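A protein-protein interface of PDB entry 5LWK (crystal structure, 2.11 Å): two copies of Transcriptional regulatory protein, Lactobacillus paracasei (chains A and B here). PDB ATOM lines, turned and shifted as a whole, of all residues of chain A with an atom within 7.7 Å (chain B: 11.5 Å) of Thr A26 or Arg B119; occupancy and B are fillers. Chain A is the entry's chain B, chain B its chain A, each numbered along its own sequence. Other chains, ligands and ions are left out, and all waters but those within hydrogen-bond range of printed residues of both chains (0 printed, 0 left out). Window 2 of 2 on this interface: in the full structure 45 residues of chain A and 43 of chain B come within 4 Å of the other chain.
NH2 of Arg B119 sits at hydrogen-bond distance from OG1 of Thr A26 (2.5 Å).
OG1 of Thr A2 lies within hydrogen-bond range of NH2 of Arg B119 (3.4 Å).
No position is printed for both chains.
Of the 12 pairs that touch across the chains among the printed residues, none has its exchanged pair printed and touching as well.
Of the 17 printed residues of chain A, 8 touch a printed residue of chain B.
Printed residues of chain A that touch a printed residue of chain B: Thr A2, Tyr A20, Ile A24, Thr A26, Phe A27, Gln A49, Leu A50 and Ile A79.
Hydrophobic or aromatic side chains of chain A that line the printed part of chain B: Tyr A20, Ile A24, Phe A27, Leu A50 and Ile A79.
Among the printed residues, no Asp or Glu carboxylate lies within 4 Å of a Lys or Arg side-chain nitrogen of the other chain.
Thr A26 touches just one residue of chain B: Arg B119 (2.5 Å).
No residue of chain B comes within 4 Å of Met A1.
Printed residues of chain B within 4 Å of Thr A2: Tyr B118 (3.3 Å) and Arg B119 (3.4 Å).
Gly A25 touches none of the printed residues of chain B.
No residue of chain B comes within 4 Å of Asp A28.
Of the printed residues of chain B, Ile A24 touches Ile B115.
Of the printed residues of chain A, Ile B115 touches Ile A24 (3.9 Å) and Phe A27 (3.7 Å).
The nearest residue of chain B that does not touch Thr A26 is Ile B115 (5.3 Å).
The nearest residue of chain A that does not touch Arg B119 is Met A1 (6.0 Å).
The nearest printed residue of chain B that does not touch Ile A24 is Phe B111 (4.02 Å).
Thr A2 touches Tyr B118 (CG2 to OH, 3.3 Å).
Phe B111 touches Tyr A20.
CD1 of Ile A24 touches CG1 of Ile B115 (3.9 Å).
CG2 of Ile B115 touches CZ of Phe A27, 3.7 Å away.
Arg B119 touches Phe A27 (NH2 to CE1, 3.4 Å).
OH of Tyr B118 touches CB of Gln A49, 3.8 Å away.
CD1 of Tyr B118 touches CD1 of Leu A50, 3.98 Å away.
CG1 of Ile A79 touches CB of Ile B99, at 3.7 Å.
Ile A79 touches Asp B100.
Ser B114 touches Ile A79 (O to CD1, 3.5 Å).
OG of Ser B114 lies within hydrogen-bond range of O of Phe B111 (2.8 Å).
OD2 of Asp B100 is in salt-bridge range of NH1 of Arg B110, 2.9 Å away.
The guanidinium group (NH1) of Arg B117 is in salt-bridge range of the side-chain carboxylate (OD2) of Asp B100, at 3.0 Å.
The backbone carbonyl oxygen (O) of Thr A2 is in hydrogen-bond range of the backbone NH (N) of Asp A28.
The backbone NH (N) of Asn A3 sits at hydrogen-bond distance from the side-chain amide oxygen (OE1) of Gln A49 (2.8 Å).
The backbone carbonyl oxygen (O) of Asn A3 lies within hydrogen-bond range of the backbone NH (N) of Leu A50 (3.1 Å).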
ATOM      1  N   MET A   1      -7.800   8.024  -5.057  1.00  0.00           N
ATOM      2  CA  MET A   1      -7.024   7.308  -6.132  1.00  0.00           C
ATOM      3  C   MET A   1      -7.800   7.034  -7.440  1.00  0.00           C
ATOM      4  O   MET A   1      -7.180   6.824  -8.484  1.00  0.00           O
ATOM      5  CB  MET A   1      -6.455   5.996  -5.577  1.00  0.00           C
ATOM      6  CG  MET A   1      -5.281   5.427  -6.360  1.00  0.00           C
ATOM      7  SD  MET A   1      -4.749   3.846  -5.681  1.00  0.00           S
ATOM      8  CE  MET A   1      -6.056   2.759  -6.250  1.00  0.00           C
ATOM      9  N   THR A   2      -9.133   7.015  -7.385  1.00  0.00           N
ATOM     10  CA  THR A   2      -9.957   6.857  -8.580  1.00  0.00           C
ATOM     11  C   THR A   2     -10.639   8.171  -8.974  1.00  0.00           C
ATOM     12  O   THR A   2     -11.332   8.799  -8.168  1.00  0.00           O
ATOM     13  CB  THR A   2     -11.012   5.758  -8.380  1.00  0.00           C
ATOM     14  OG1 THR A   2     -11.813   6.061  -7.236  1.00  0.00           O
ATOM     15  CG2 THR A   2     -10.332   4.407  -8.180  1.00  0.00           C
ATOM     16  N   ASN A   3     -10.453   8.529 -10.241  1.00  0.00           N
ATOM     17  CA  ASN A   3     -11.057   9.709 -10.826  1.00  0.00           C
ATOM     18  C   ASN A   3     -12.357   9.253 -11.478  1.00  0.00           C
ATOM     19  O   ASN A   3     -12.472   8.113 -11.928  1.00  0.00           O
ATOM     20  CB  ASN A   3     -10.129  10.334 -11.867  1.00  0.00           C
ATOM     21  CG  ASN A   3      -8.822  10.816 -11.268  1.00  0.00           C
ATOM     22  OD1 ASN A   3      -8.813  11.584 -10.306  1.00  0.00           O
ATOM     23  ND2 ASN A   3      -7.709  10.365 -11.834  1.00  0.00           N
ATOM     24  N   ILE A   4     -13.334  10.147 -11.520  1.00  0.00           N
ATOM     25  CA  ILE A   4     -14.651   9.862 -12.089  1.00  0.00           C
ATOM     26  C   ILE A   4     -15.037  10.863 -13.175  1.00  0.00           C
ATOM     27  O   ILE A   4     -14.787  12.064 -13.041  1.00  0.00           O
ATOM     28  CB  ILE A   4     -15.726   9.881 -10.990  1.00  0.00           C
ATOM     29  CG1 ILE A   4     -15.475   8.722 -10.030  1.00  0.00           C
ATOM     30  CG2 ILE A   4     -17.140   9.775 -11.574  1.00  0.00           C
ATOM     31  CD1 ILE A   4     -16.189   8.893  -8.724  1.00  0.00           C
ATOM     32  N   TYR A  20     -23.466  12.465  -4.056  1.00  0.00           N
ATOM     33  CA  TYR A  20     -23.376  11.088  -3.575  1.00  0.00           C
ATOM     34  C   TYR A  20     -21.943  10.563  -3.568  1.00  0.00           C
ATOM     35  O   TYR A  20     -21.546   9.875  -2.632  1.00  0.00           O
ATOM     36  CB  TYR A  20     -24.301  10.185  -4.405  1.00  0.00           C
ATOM     37  CG  TYR A  20     -25.792  10.320  -4.092  1.00  0.00           C
ATOM     38  CD1 TYR A  20     -26.283  11.267  -3.176  1.00  0.00           C
ATOM     39  CD2 TYR A  20     -26.721   9.501  -4.730  1.00  0.00           C
ATOM     40  CE1 TYR A  20     -27.643  11.366  -2.899  1.00  0.00           C
ATOM     41  CE2 TYR A  20     -28.083   9.605  -4.461  1.00  0.00           C
ATOM     42  CZ  TYR A  20     -28.535  10.536  -3.545  1.00  0.00           C
ATOM     43  OH  TYR A  20     -29.883  10.640  -3.287  1.00  0.00           O
ATOM     44  N   LEU A  21     -21.175  10.896  -4.599  1.00  0.00           N
ATOM     45  CA  LEU A  21     -19.767  10.530  -4.655  1.00  0.00           C
ATOM     46  C   LEU A  21     -18.974  11.182  -3.519  1.00  0.00           C
ATOM     47  O   LEU A  21     -18.077  10.556  -2.948  1.00  0.00           O
ATOM     48  CB  LEU A  21     -19.164  10.911  -6.009  1.00  0.00           C
ATOM     49  CG  LEU A  21     -19.705  10.122  -7.209  1.00  0.00           C
ATOM     50  CD1 LEU A  21     -19.285  10.771  -8.517  1.00  0.00           C
ATOM     51  CD2 LEU A  21     -19.273   8.662  -7.150  1.00  0.00           C
ATOM     52  N   GLU A  22     -19.316  12.431  -3.200  1.00  0.00           N
ATOM     53  CA  GLU A  22     -18.679  13.171  -2.105  1.00  0.00           C
ATOM     54  C   GLU A  22     -19.021  12.585  -0.744  1.00  0.00           C
ATOM     55  O   GLU A  22     -18.157  12.496   0.119  1.00  0.00           O
ATOM     56  CB  GLU A  22     -19.055  14.651  -2.157  1.00  0.00           C
ATOM     57  CG  GLU A  22     -18.362  15.383  -3.299  1.00  0.00           C
ATOM     58  CD  GLU A  22     -18.784  16.836  -3.453  1.00  0.00           C
ATOM     59  OE1 GLU A  22     -19.523  17.363  -2.589  1.00  0.00           O
ATOM     60  OE2 GLU A  22     -18.366  17.459  -4.455  1.00  0.00           O
ATOM     61  N   LYS A  23     -20.275  12.182  -0.568  1.00  0.00           N
ATOM     62  CA  LYS A  23     -20.705  11.488   0.650  1.00  0.00           C
ATOM     63  C   LYS A  23     -19.910  10.215   0.918  1.00  0.00           C
ATOM     64  O   LYS A  23     -19.466   9.974   2.037  1.00  0.00           O
ATOM     65  CB  LYS A  23     -22.197  11.149   0.606  1.00  0.00           C
ATOM     66  CG  LYS A  23     -23.040  12.094   1.438  1.00  0.00           C
ATOM     67  CD  LYS A  23     -24.479  11.618   1.585  1.00  0.00           C
ATOM     68  CE  LYS A  23     -24.926  11.716   3.037  1.00  0.00           C
ATOM     69  NZ  LYS A  23     -26.372  11.430   3.235  1.00  0.00           N
ATOM     70  N   ILE A  24     -19.742   9.410  -0.123  1.00  0.00           N
ATOM     71  CA  ILE A  24     -18.944   8.189  -0.037  1.00  0.00           C
ATOM     72  C   ILE A  24     -17.462   8.532   0.153  1.00  0.00           C
ATOM     73  O   ILE A  24     -16.742   7.818   0.842  1.00  0.00           O
ATOM     74  CB  ILE A  24     -19.153   7.318  -1.288  1.00  0.00           C
ATOM     75  CG1 ILE A  24     -20.620   6.860  -1.359  1.00  0.00           C
ATOM     76  CG2 ILE A  24     -18.238   6.098  -1.274  1.00  0.00           C
ATOM     77  CD1 ILE A  24     -21.087   6.540  -2.763  1.00  0.00           C
ATOM     78  N   GLY A  25     -17.023   9.612  -0.489  1.00  0.00           N
ATOM     79  CA  GLY A  25     -15.750  10.261  -0.197  1.00  0.00           C
ATOM     80  C   GLY A  25     -14.443   9.545  -0.473  1.00  0.00           C
ATOM     81  O   GLY A  25     -13.427   9.921   0.109  1.00  0.00           O
ATOM     82  N   THR A  26     -14.432   8.554  -1.365  1.00  0.00           N
ATOM     83  CA  THR A  26     -13.190   7.809  -1.664  1.00  0.00           C
ATOM     84  C   THR A  26     -12.628   8.080  -3.067  1.00  0.00           C
ATOM     85  O   THR A  26     -11.881   7.256  -3.612  1.00  0.00           O
ATOM     86  CB  THR A  26     -13.393   6.289  -1.477  1.00  0.00           C
ATOM     87  OG1 THR A  26     -14.349   5.810  -2.433  1.00  0.00           O
ATOM     88  CG2 THR A  26     -13.911   5.985  -0.080  1.00  0.00           C
ATOM     89  N   PHE A  27     -12.963   9.242  -3.631  1.00  0.00           N
ATOM     90  CA  PHE A  27     -12.584   9.595  -5.000  1.00  0.00           C
ATOM     91  C   PHE A  27     -11.789  10.897  -5.042  1.00  0.00           C
ATOM     92  O   PHE A  27     -11.862  11.701  -4.108  1.00  0.00           O
ATOM     93  CB  PHE A  27     -13.843   9.732  -5.843  1.00  0.00           C
ATOM     94  CG  PHE A  27     -14.798   8.588  -5.685  1.00  0.00           C
ATOM     95  CD1 PHE A  27     -14.597   7.406  -6.382  1.00  0.00           C
ATOM     96  CD2 PHE A  27     -15.886   8.685  -4.827  1.00  0.00           C
ATOM     97  CE1 PHE A  27     -15.479   6.349  -6.248  1.00  0.00           C
ATOM     98  CE2 PHE A  27     -16.766   7.630  -4.680  1.00  0.00           C
ATOM     99  CZ  PHE A  27     -16.563   6.461  -5.391  1.00  0.00           C
ATOM    100  N   ASP A  28     -11.050  11.108  -6.131  1.00  0.00           N
ATOM    101  CA  ASP A  28     -10.165  12.283  -6.264  1.00  0.00           C
ATOM    102  C   ASP A  28     -10.795  13.472  -7.001  1.00  0.00           C
ATOM    103  O   ASP A  28     -11.192  14.455  -6.379  1.00  0.00           O
ATOM    104  CB  ASP A  28      -8.843  11.883  -6.944  1.00  0.00           C
ATOM    105  CG  ASP A  28      -7.911  11.112  -6.026  1.00  0.00           C
ATOM    106  OD1 ASP A  28      -8.355  10.620  -4.964  1.00  0.00           O
ATOM    107  OD2 ASP A  28      -6.719  10.982  -6.380  1.00  0.00           O
ATOM    108  N   THR A  29     -10.900  13.358  -8.316  1.00  0.00           N
ATOM    109  CA  THR A  29     -11.296  14.448  -9.203  1.00  0.00           C
ATOM    110  C   THR A  29     -12.538  13.948  -9.915  1.00  0.00           C
ATOM    111  O   THR A  29     -12.523  12.863 -10.515  1.00  0.00           O
ATOM    112  CB  THR A  29     -10.252  14.791 -10.286  1.00  0.00           C
ATOM    113  OG1 THR A  29      -8.965  14.966  -9.690  1.00  0.00           O
ATOM    114  CG2 THR A  29     -10.653  16.077 -11.013  1.00  0.00           C
ATOM    115  N   GLN A  49     -10.771   6.744 -14.114  1.00  0.00           N
ATOM    116  CA  GLN A  49     -10.928   5.344 -13.844  1.00  0.00           C
ATOM    117  C   GLN A  49     -12.359   4.817 -13.885  1.00  0.00           C
ATOM    118  O   GLN A  49     -12.575   3.677 -14.166  1.00  0.00           O
ATOM    119  CB  GLN A  49     -10.296   5.038 -12.503  1.00  0.00           C
ATOM    120  CG  GLN A  49      -8.786   5.108 -12.508  1.00  0.00           C
ATOM    121  CD  GLN A  49      -8.277   6.495 -12.745  1.00  0.00           C
ATOM    122  OE1 GLN A  49      -8.505   7.373 -11.962  1.00  0.00           O
ATOM    123  NE2 GLN A  49      -7.599   6.689 -13.841  1.00  0.00           N
ATOM    124  N   LEU A  50     -13.333   5.660 -13.603  1.00  0.00           N
ATOM    125  CA  LEU A  50     -14.722   5.257 -13.627  1.00  0.00           C
ATOM    126  C   LEU A  50     -15.643   6.271 -14.269  1.00  0.00           C
ATOM    127  O   LEU A  50     -15.504   7.444 -14.055  1.00  0.00           O
ATOM    128  CB  LEU A  50     -15.196   4.960 -12.214  1.00  0.00           C
ATOM    129  CG  LEU A  50     -16.663   4.660 -11.964  1.00  0.00           C
ATOM    130  CD1 LEU A  50     -17.090   3.332 -12.525  1.00  0.00           C
ATOM    131  CD2 LEU A  50     -16.985   4.732 -10.498  1.00  0.00           C
ATOM    132  N   ILE A  79     -20.545   2.526 -15.114  1.00  0.00           N
ATOM    133  CA  ILE A  79     -21.777   2.261 -14.442  1.00  0.00           C
ATOM    134  C   ILE A  79     -22.814   3.052 -15.201  1.00  0.00           C
ATOM    135  O   ILE A  79     -22.652   4.220 -15.412  1.00  0.00           O
ATOM    136  CB  ILE A  79     -21.765   2.712 -12.981  1.00  0.00           C
ATOM    137  CG1 ILE A  79     -20.803   1.864 -12.179  1.00  0.00           C
ATOM    138  CG2 ILE A  79     -23.153   2.628 -12.399  1.00  0.00           C
ATOM    139  CD1 ILE A  79     -20.713   2.254 -10.737  1.00  0.00           C
ATOM    140  N   VAL B  98     -20.410  -3.590 -18.061  1.00  0.00           N
ATOM    141  CA  VAL B  98     -20.618  -2.547 -17.095  1.00  0.00           C
ATOM    142  C   VAL B  98     -20.638  -3.112 -15.688  1.00  0.00           C
ATOM    143  O   VAL B  98     -21.024  -4.232 -15.479  1.00  0.00           O
ATOM    144  CB  VAL B  98     -21.919  -1.775 -17.342  1.00  0.00           C
ATOM    145  CG1 VAL B  98     -21.928  -1.156 -18.709  1.00  0.00           C
ATOM    146  CG2 VAL B  98     -23.126  -2.641 -17.106  1.00  0.00           C
ATOM    147  N   ILE B  99     -20.202  -2.313 -14.735  1.00  0.00           N
ATOM    148  CA  ILE B  99     -20.213  -2.678 -13.344  1.00  0.00           C
ATOM    149  C   ILE B  99     -21.633  -2.830 -12.833  1.00  0.00           C
ATOM    150  O   ILE B  99     -21.922  -3.727 -12.096  1.00  0.00           O
ATOM    151  CB  ILE B  99     -19.525  -1.606 -12.502  1.00  0.00           C
ATOM    152  CG1 ILE B  99     -18.070  -1.421 -12.909  1.00  0.00           C
ATOM    153  CG2 ILE B  99     -19.628  -1.909 -11.027  1.00  0.00           C
ATOM    154  CD1 ILE B  99     -17.267  -2.677 -12.986  1.00  0.00           C
ATOM    155  N   ASP B 100     -22.508  -1.923 -13.225  1.00  0.00           N
ATOM    156  CA  ASP B 100     -23.888  -1.924 -12.788  1.00  0.00           C
ATOM    157  C   ASP B 100     -24.797  -1.147 -13.708  1.00  0.00           C
ATOM    158  O   ASP B 100     -24.351  -0.418 -14.531  1.00  0.00           O
ATOM    159  CB  ASP B 100     -23.966  -1.318 -11.401  1.00  0.00           C
ATOM    160  CG  ASP B 100     -25.072  -1.887 -10.571  1.00  0.00           C
ATOM    161  OD1 ASP B 100     -25.925  -2.581 -11.081  1.00  0.00           O
ATOM    162  OD2 ASP B 100     -25.101  -1.634  -9.382  1.00  0.00           O
ATOM    163  N   ARG B 110     -29.056   2.496  -3.208  1.00  0.00           N
ATOM    164  CA  ARG B 110     -28.827   1.812  -4.464  1.00  0.00           C
ATOM    165  C   ARG B 110     -27.579   2.346  -5.110  1.00  0.00           C
ATOM    166  O   ARG B 110     -26.827   1.606  -5.685  1.00  0.00           O
ATOM    167  CB  ARG B 110     -30.030   1.880  -5.381  1.00  0.00           C
ATOM    168  CG  ARG B 110     -29.887   1.085  -6.655  1.00  0.00           C
ATOM    169  CD  ARG B 110     -29.814  -0.404  -6.425  1.00  0.00           C
ATOM    170  NE  ARG B 110     -29.757  -1.142  -7.665  1.00  0.00           N
ATOM    171  CZ  ARG B 110     -28.659  -1.366  -8.360  1.00  0.00           C
ATOM    172  NH1 ARG B 110     -27.511  -0.895  -7.963  1.00  0.00           N
ATOM    173  NH2 ARG B 110     -28.720  -2.055  -9.466  1.00  0.00           N
ATOM    174  N   PHE B 111     -27.364   3.644  -5.011  1.00  0.00           N
ATOM    175  CA  PHE B 111     -26.189   4.244  -5.594  1.00  0.00           C
ATOM    176  C   PHE B 111     -24.925   3.691  -4.954  1.00  0.00           C
ATOM    177  O   PHE B 111     -24.011   3.331  -5.637  1.00  0.00           O
ATOM    178  CB  PHE B 111     -26.262   5.752  -5.433  1.00  0.00           C
ATOM    179  CG  PHE B 111     -25.185   6.498  -6.142  1.00  0.00           C
ATOM    180  CD1 PHE B 111     -25.420   7.091  -7.358  1.00  0.00           C
ATOM    181  CD2 PHE B 111     -23.949   6.629  -5.585  1.00  0.00           C
ATOM    182  CE1 PHE B 111     -24.435   7.782  -8.009  1.00  0.00           C
ATOM    183  CE2 PHE B 111     -22.957   7.317  -6.231  1.00  0.00           C
ATOM    184  CZ  PHE B 111     -23.201   7.897  -7.446  1.00  0.00           C
ATOM    185  N   GLU B 112     -24.918   3.579  -3.636  1.00  0.00           N
ATOM    186  CA  GLU B 112     -23.787   3.064  -2.887  1.00  0.00           C
ATOM    187  C   GLU B 112     -23.472   1.637  -3.270  1.00  0.00           C
ATOM    188  O   GLU B 112     -22.343   1.278  -3.410  1.00  0.00           O
ATOM    189  CB  GLU B 112     -24.096   3.101  -1.406  1.00  0.00           C
ATOM    190  CG  GLU B 112     -23.931   4.426  -0.709  1.00  0.00           C
ATOM    191  CD  GLU B 112     -24.086   4.268   0.784  1.00  0.00           C
ATOM    192  OE1 GLU B 112     -25.134   4.638   1.311  1.00  0.00           O
ATOM    193  OE2 GLU B 112     -23.171   3.733   1.422  1.00  0.00           O
ATOM    194  N   LYS B 113     -24.496   0.828  -3.433  1.00  0.00           N
ATOM    195  CA  LYS B 113     -24.360  -0.559  -3.908  1.00  0.00           C
ATOM    196  C   LYS B 113     -23.568  -0.636  -5.211  1.00  0.00           C
ATOM    197  O   LYS B 113     -22.662  -1.463  -5.336  1.00  0.00           O
ATOM    198  CB  LYS B 113     -25.733  -1.205  -4.120  1.00  0.00           C
ATOM    199  CG  LYS B 113     -25.714  -2.705  -4.413  1.00  0.00           C
ATOM    200  CD  LYS B 113     -25.670  -3.524  -3.133  1.00  0.00           C
ATOM    201  CE  LYS B 113     -25.753  -5.018  -3.409  1.00  0.00           C
ATOM    202  NZ  LYS B 113     -24.467  -5.583  -3.910  1.00  0.00           N
ATOM    203  N   SER B 114     -23.900   0.223  -6.176  1.00  0.00           N
ATOM    204  CA  SER B 114     -23.170   0.226  -7.453  1.00  0.00           C
ATOM    205  C   SER B 114     -21.684   0.565  -7.269  1.00  0.00           C
ATOM    206  O   SER B 114     -20.832   0.040  -7.985  1.00  0.00           O
ATOM    207  CB  SER B 114     -23.829   1.166  -8.470  1.00  0.00           C
ATOM    208  OG  SER B 114     -23.458   2.519  -8.275  1.00  0.00           O
ATOM    209  N   ILE B 115     -21.385   1.418  -6.292  1.00  0.00           N
ATOM    210  CA  ILE B 115     -20.002   1.782  -5.964  1.00  0.00           C
ATOM    211  C   ILE B 115     -19.281   0.620  -5.269  1.00  0.00           C
ATOM    212  O   ILE B 115     -18.146   0.308  -5.621  1.00  0.00           O
ATOM    213  CB  ILE B 115     -19.936   3.070  -5.109  1.00  0.00           C
ATOM    214  CG1 ILE B 115     -20.573   4.263  -5.852  1.00  0.00           C
ATOM    215  CG2 ILE B 115     -18.501   3.398  -4.707  1.00  0.00           C
ATOM    216  CD1 ILE B 115     -19.904   4.687  -7.146  1.00  0.00           C
ATOM    217  N   GLN B 116     -19.944  -0.028  -4.308  1.00  0.00           N
ATOM    218  CA  GLN B 116     -19.412  -1.263  -3.702  1.00  0.00           C
ATOM    219  C   GLN B 116     -19.041  -2.281  -4.770  1.00  0.00           C
ATOM    220  O   GLN B 116     -17.976  -2.883  -4.701  1.00  0.00           O
ATOM    221  CB  GLN B 116     -20.416  -1.904  -2.742  1.00  0.00           C
ATOM    222  CG  GLN B 116     -20.644  -1.138  -1.450  1.00  0.00           C
ATOM    223  CD  GLN B 116     -21.886  -1.625  -0.712  1.00  0.00           C
ATOM    224  OE1 GLN B 116     -22.135  -2.833  -0.630  1.00  0.00           O
ATOM    225  NE2 GLN B 116     -22.676  -0.691  -0.180  1.00  0.00           N
ATOM    226  N   ARG B 117     -19.912  -2.455  -5.761  1.00  0.00           N
ATOM    227  CA  ARG B 117     -19.642  -3.394  -6.856  1.00  0.00           C
ATOM    228  C   ARG B 117     -18.399  -3.025  -7.663  1.00  0.00           C
ATOM    229  O   ARG B 117     -17.662  -3.908  -8.092  1.00  0.00           O
ATOM    230  CB  ARG B 117     -20.853  -3.541  -7.770  1.00  0.00           C
ATOM    231  CG  ARG B 117     -22.000  -4.281  -7.106  1.00  0.00           C
ATOM    232  CD  ARG B 117     -23.199  -4.372  -8.025  1.00  0.00           C
ATOM    233  NE  ARG B 117     -24.206  -5.300  -7.501  1.00  0.00           N
ATOM    234  CZ  ARG B 117     -25.515  -5.059  -7.356  1.00  0.00           C
ATOM    235  NH1 ARG B 117     -26.068  -3.896  -7.709  1.00  0.00           N
ATOM    236  NH2 ARG B 117     -26.299  -6.014  -6.859  1.00  0.00           N
ATOM    237  N   TYR B 118     -18.168  -1.729  -7.865  1.00  0.00           N
ATOM    238  CA  TYR B 118     -16.923  -1.265  -8.488  1.00  0.00           C
ATOM    239  C   TYR B 118     -15.694  -1.602  -7.624  1.00  0.00           C
ATOM    240  O   TYR B 118     -14.682  -2.084  -8.142  1.00  0.00           O
ATOM    241  CB  TYR B 118     -16.971   0.244  -8.773  1.00  0.00           C
ATOM    242  CG  TYR B 118     -15.637   0.831  -9.179  1.00  0.00           C
ATOM    243  CD1 TYR B 118     -15.101   0.590 -10.439  1.00  0.00           C
ATOM    244  CD2 TYR B 118     -14.900   1.619  -8.295  1.00  0.00           C
ATOM    245  CE1 TYR B 118     -13.869   1.120 -10.807  1.00  0.00           C
ATOM    246  CE2 TYR B 118     -13.668   2.153  -8.658  1.00  0.00           C
ATOM    247  CZ  TYR B 118     -13.157   1.901  -9.914  1.00  0.00           C
ATOM    248  OH  TYR B 118     -11.934   2.432 -10.279  1.00  0.00           O
ATOM    249  N   ARG B 119     -15.791  -1.333  -6.323  1.00  0.00           N
ATOM    250  CA  ARG B 119     -14.680  -1.571  -5.389  1.00  0.00           C
ATOM    251  C   ARG B 119     -14.323  -3.047  -5.270  1.00  0.00           C
ATOM    252  O   ARG B 119     -13.146  -3.413  -5.358  1.00  0.00           O
ATOM    253  CB  ARG B 119     -15.006  -1.005  -4.002  1.00  0.00           C
ATOM    254  CG  ARG B 119     -15.150   0.514  -3.946  1.00  0.00           C
ATOM    255  CD  ARG B 119     -13.947   1.225  -4.546  1.00  0.00           C
ATOM    256  NE  ARG B 119     -13.933   2.657  -4.265  1.00  0.00           N
ATOM    257  CZ  ARG B 119     -13.009   3.508  -4.717  1.00  0.00           C
ATOM    258  NH1 ARG B 119     -12.001   3.089  -5.479  1.00  0.00           N
ATOM    259  NH2 ARG B 119     -13.092   4.795  -4.403  1.00  0.00           N
ATOM    260  N   THR B 120     -15.336  -3.893  -5.114  1.00  0.00           N
ATOM    261  CA  THR B 120     -15.122  -5.342  -5.066  1.00  0.00           C
ATOM    262  C   THR B 120     -14.502  -5.877  -6.365  1.00  0.00           C
ATOM    263  O   THR B 120     -13.698  -6.809  -6.334  1.00  0.00           O
ATOM    264  CB  THR B 120     -16.427  -6.103  -4.766  1.00  0.00           C
ATOM    265  OG1 THR B 120     -17.426  -5.728  -5.716  1.00  0.00           O
ATOM    266  CG2 THR B 120     -16.927  -5.794  -3.357  1.00  0.00           C
ATOM    267  N   LYS B 121     -14.858  -5.275  -7.496  1.00  0.00           N
ATOM    268  CA  LYS B 121     -14.232  -5.602  -8.779  1.00  0.00           C
ATOM    269  C   LYS B 121     -12.743  -5.191  -8.858  1.00  0.00           C
ATOM    270  O   LYS B 121     -11.990  -5.782  -9.632  1.00  0.00           O
ATOM    271  CB  LYS B 121     -15.035  -4.960  -9.913  1.00  0.00           C
ATOM    272  CG  LYS B 121     -14.582  -5.317 -11.318  1.00  0.00           C
ATOM    273  CD  LYS B 121     -13.905  -4.136 -11.995  1.00  0.00           C
ATOM    274  CE  LYS B 121     -13.283  -4.531 -13.323  1.00  0.00           C
ATOM    275  NZ  LYS B 121     -12.153  -3.631 -13.683  1.00  0.00           N
ATOM    276  N   HIS B 122     -12.345  -4.196  -8.055  1.00  0.00           N
ATOM    277  CA  HIS B 122     -10.977  -3.627  -7.968  1.00  0.00           C
ATOM    278  C   HIS B 122     -10.839  -2.446  -8.921  1.00  0.00           C
ATOM    279  O   HIS B 122     -11.343  -1.360  -8.645  1.00  0.00           O
ATOM    280  CB  HIS B 122      -9.837  -4.637  -8.216  1.00  0.00           C
ATOM    281  CG  HIS B 122      -9.825  -5.797  -7.270  1.00  0.00           C
ATOM    282  ND1 HIS B 122      -9.851  -5.641  -5.900  1.00  0.00           N
ATOM    283  CD2 HIS B 122      -9.756  -7.132  -7.494  1.00  0.00           C
ATOM    284  CE1 HIS B 122      -9.815  -6.828  -5.323  1.00  0.00           C
ATOM    285  NE2 HIS B 122      -9.757  -7.750  -6.268  1.00  0.00           N
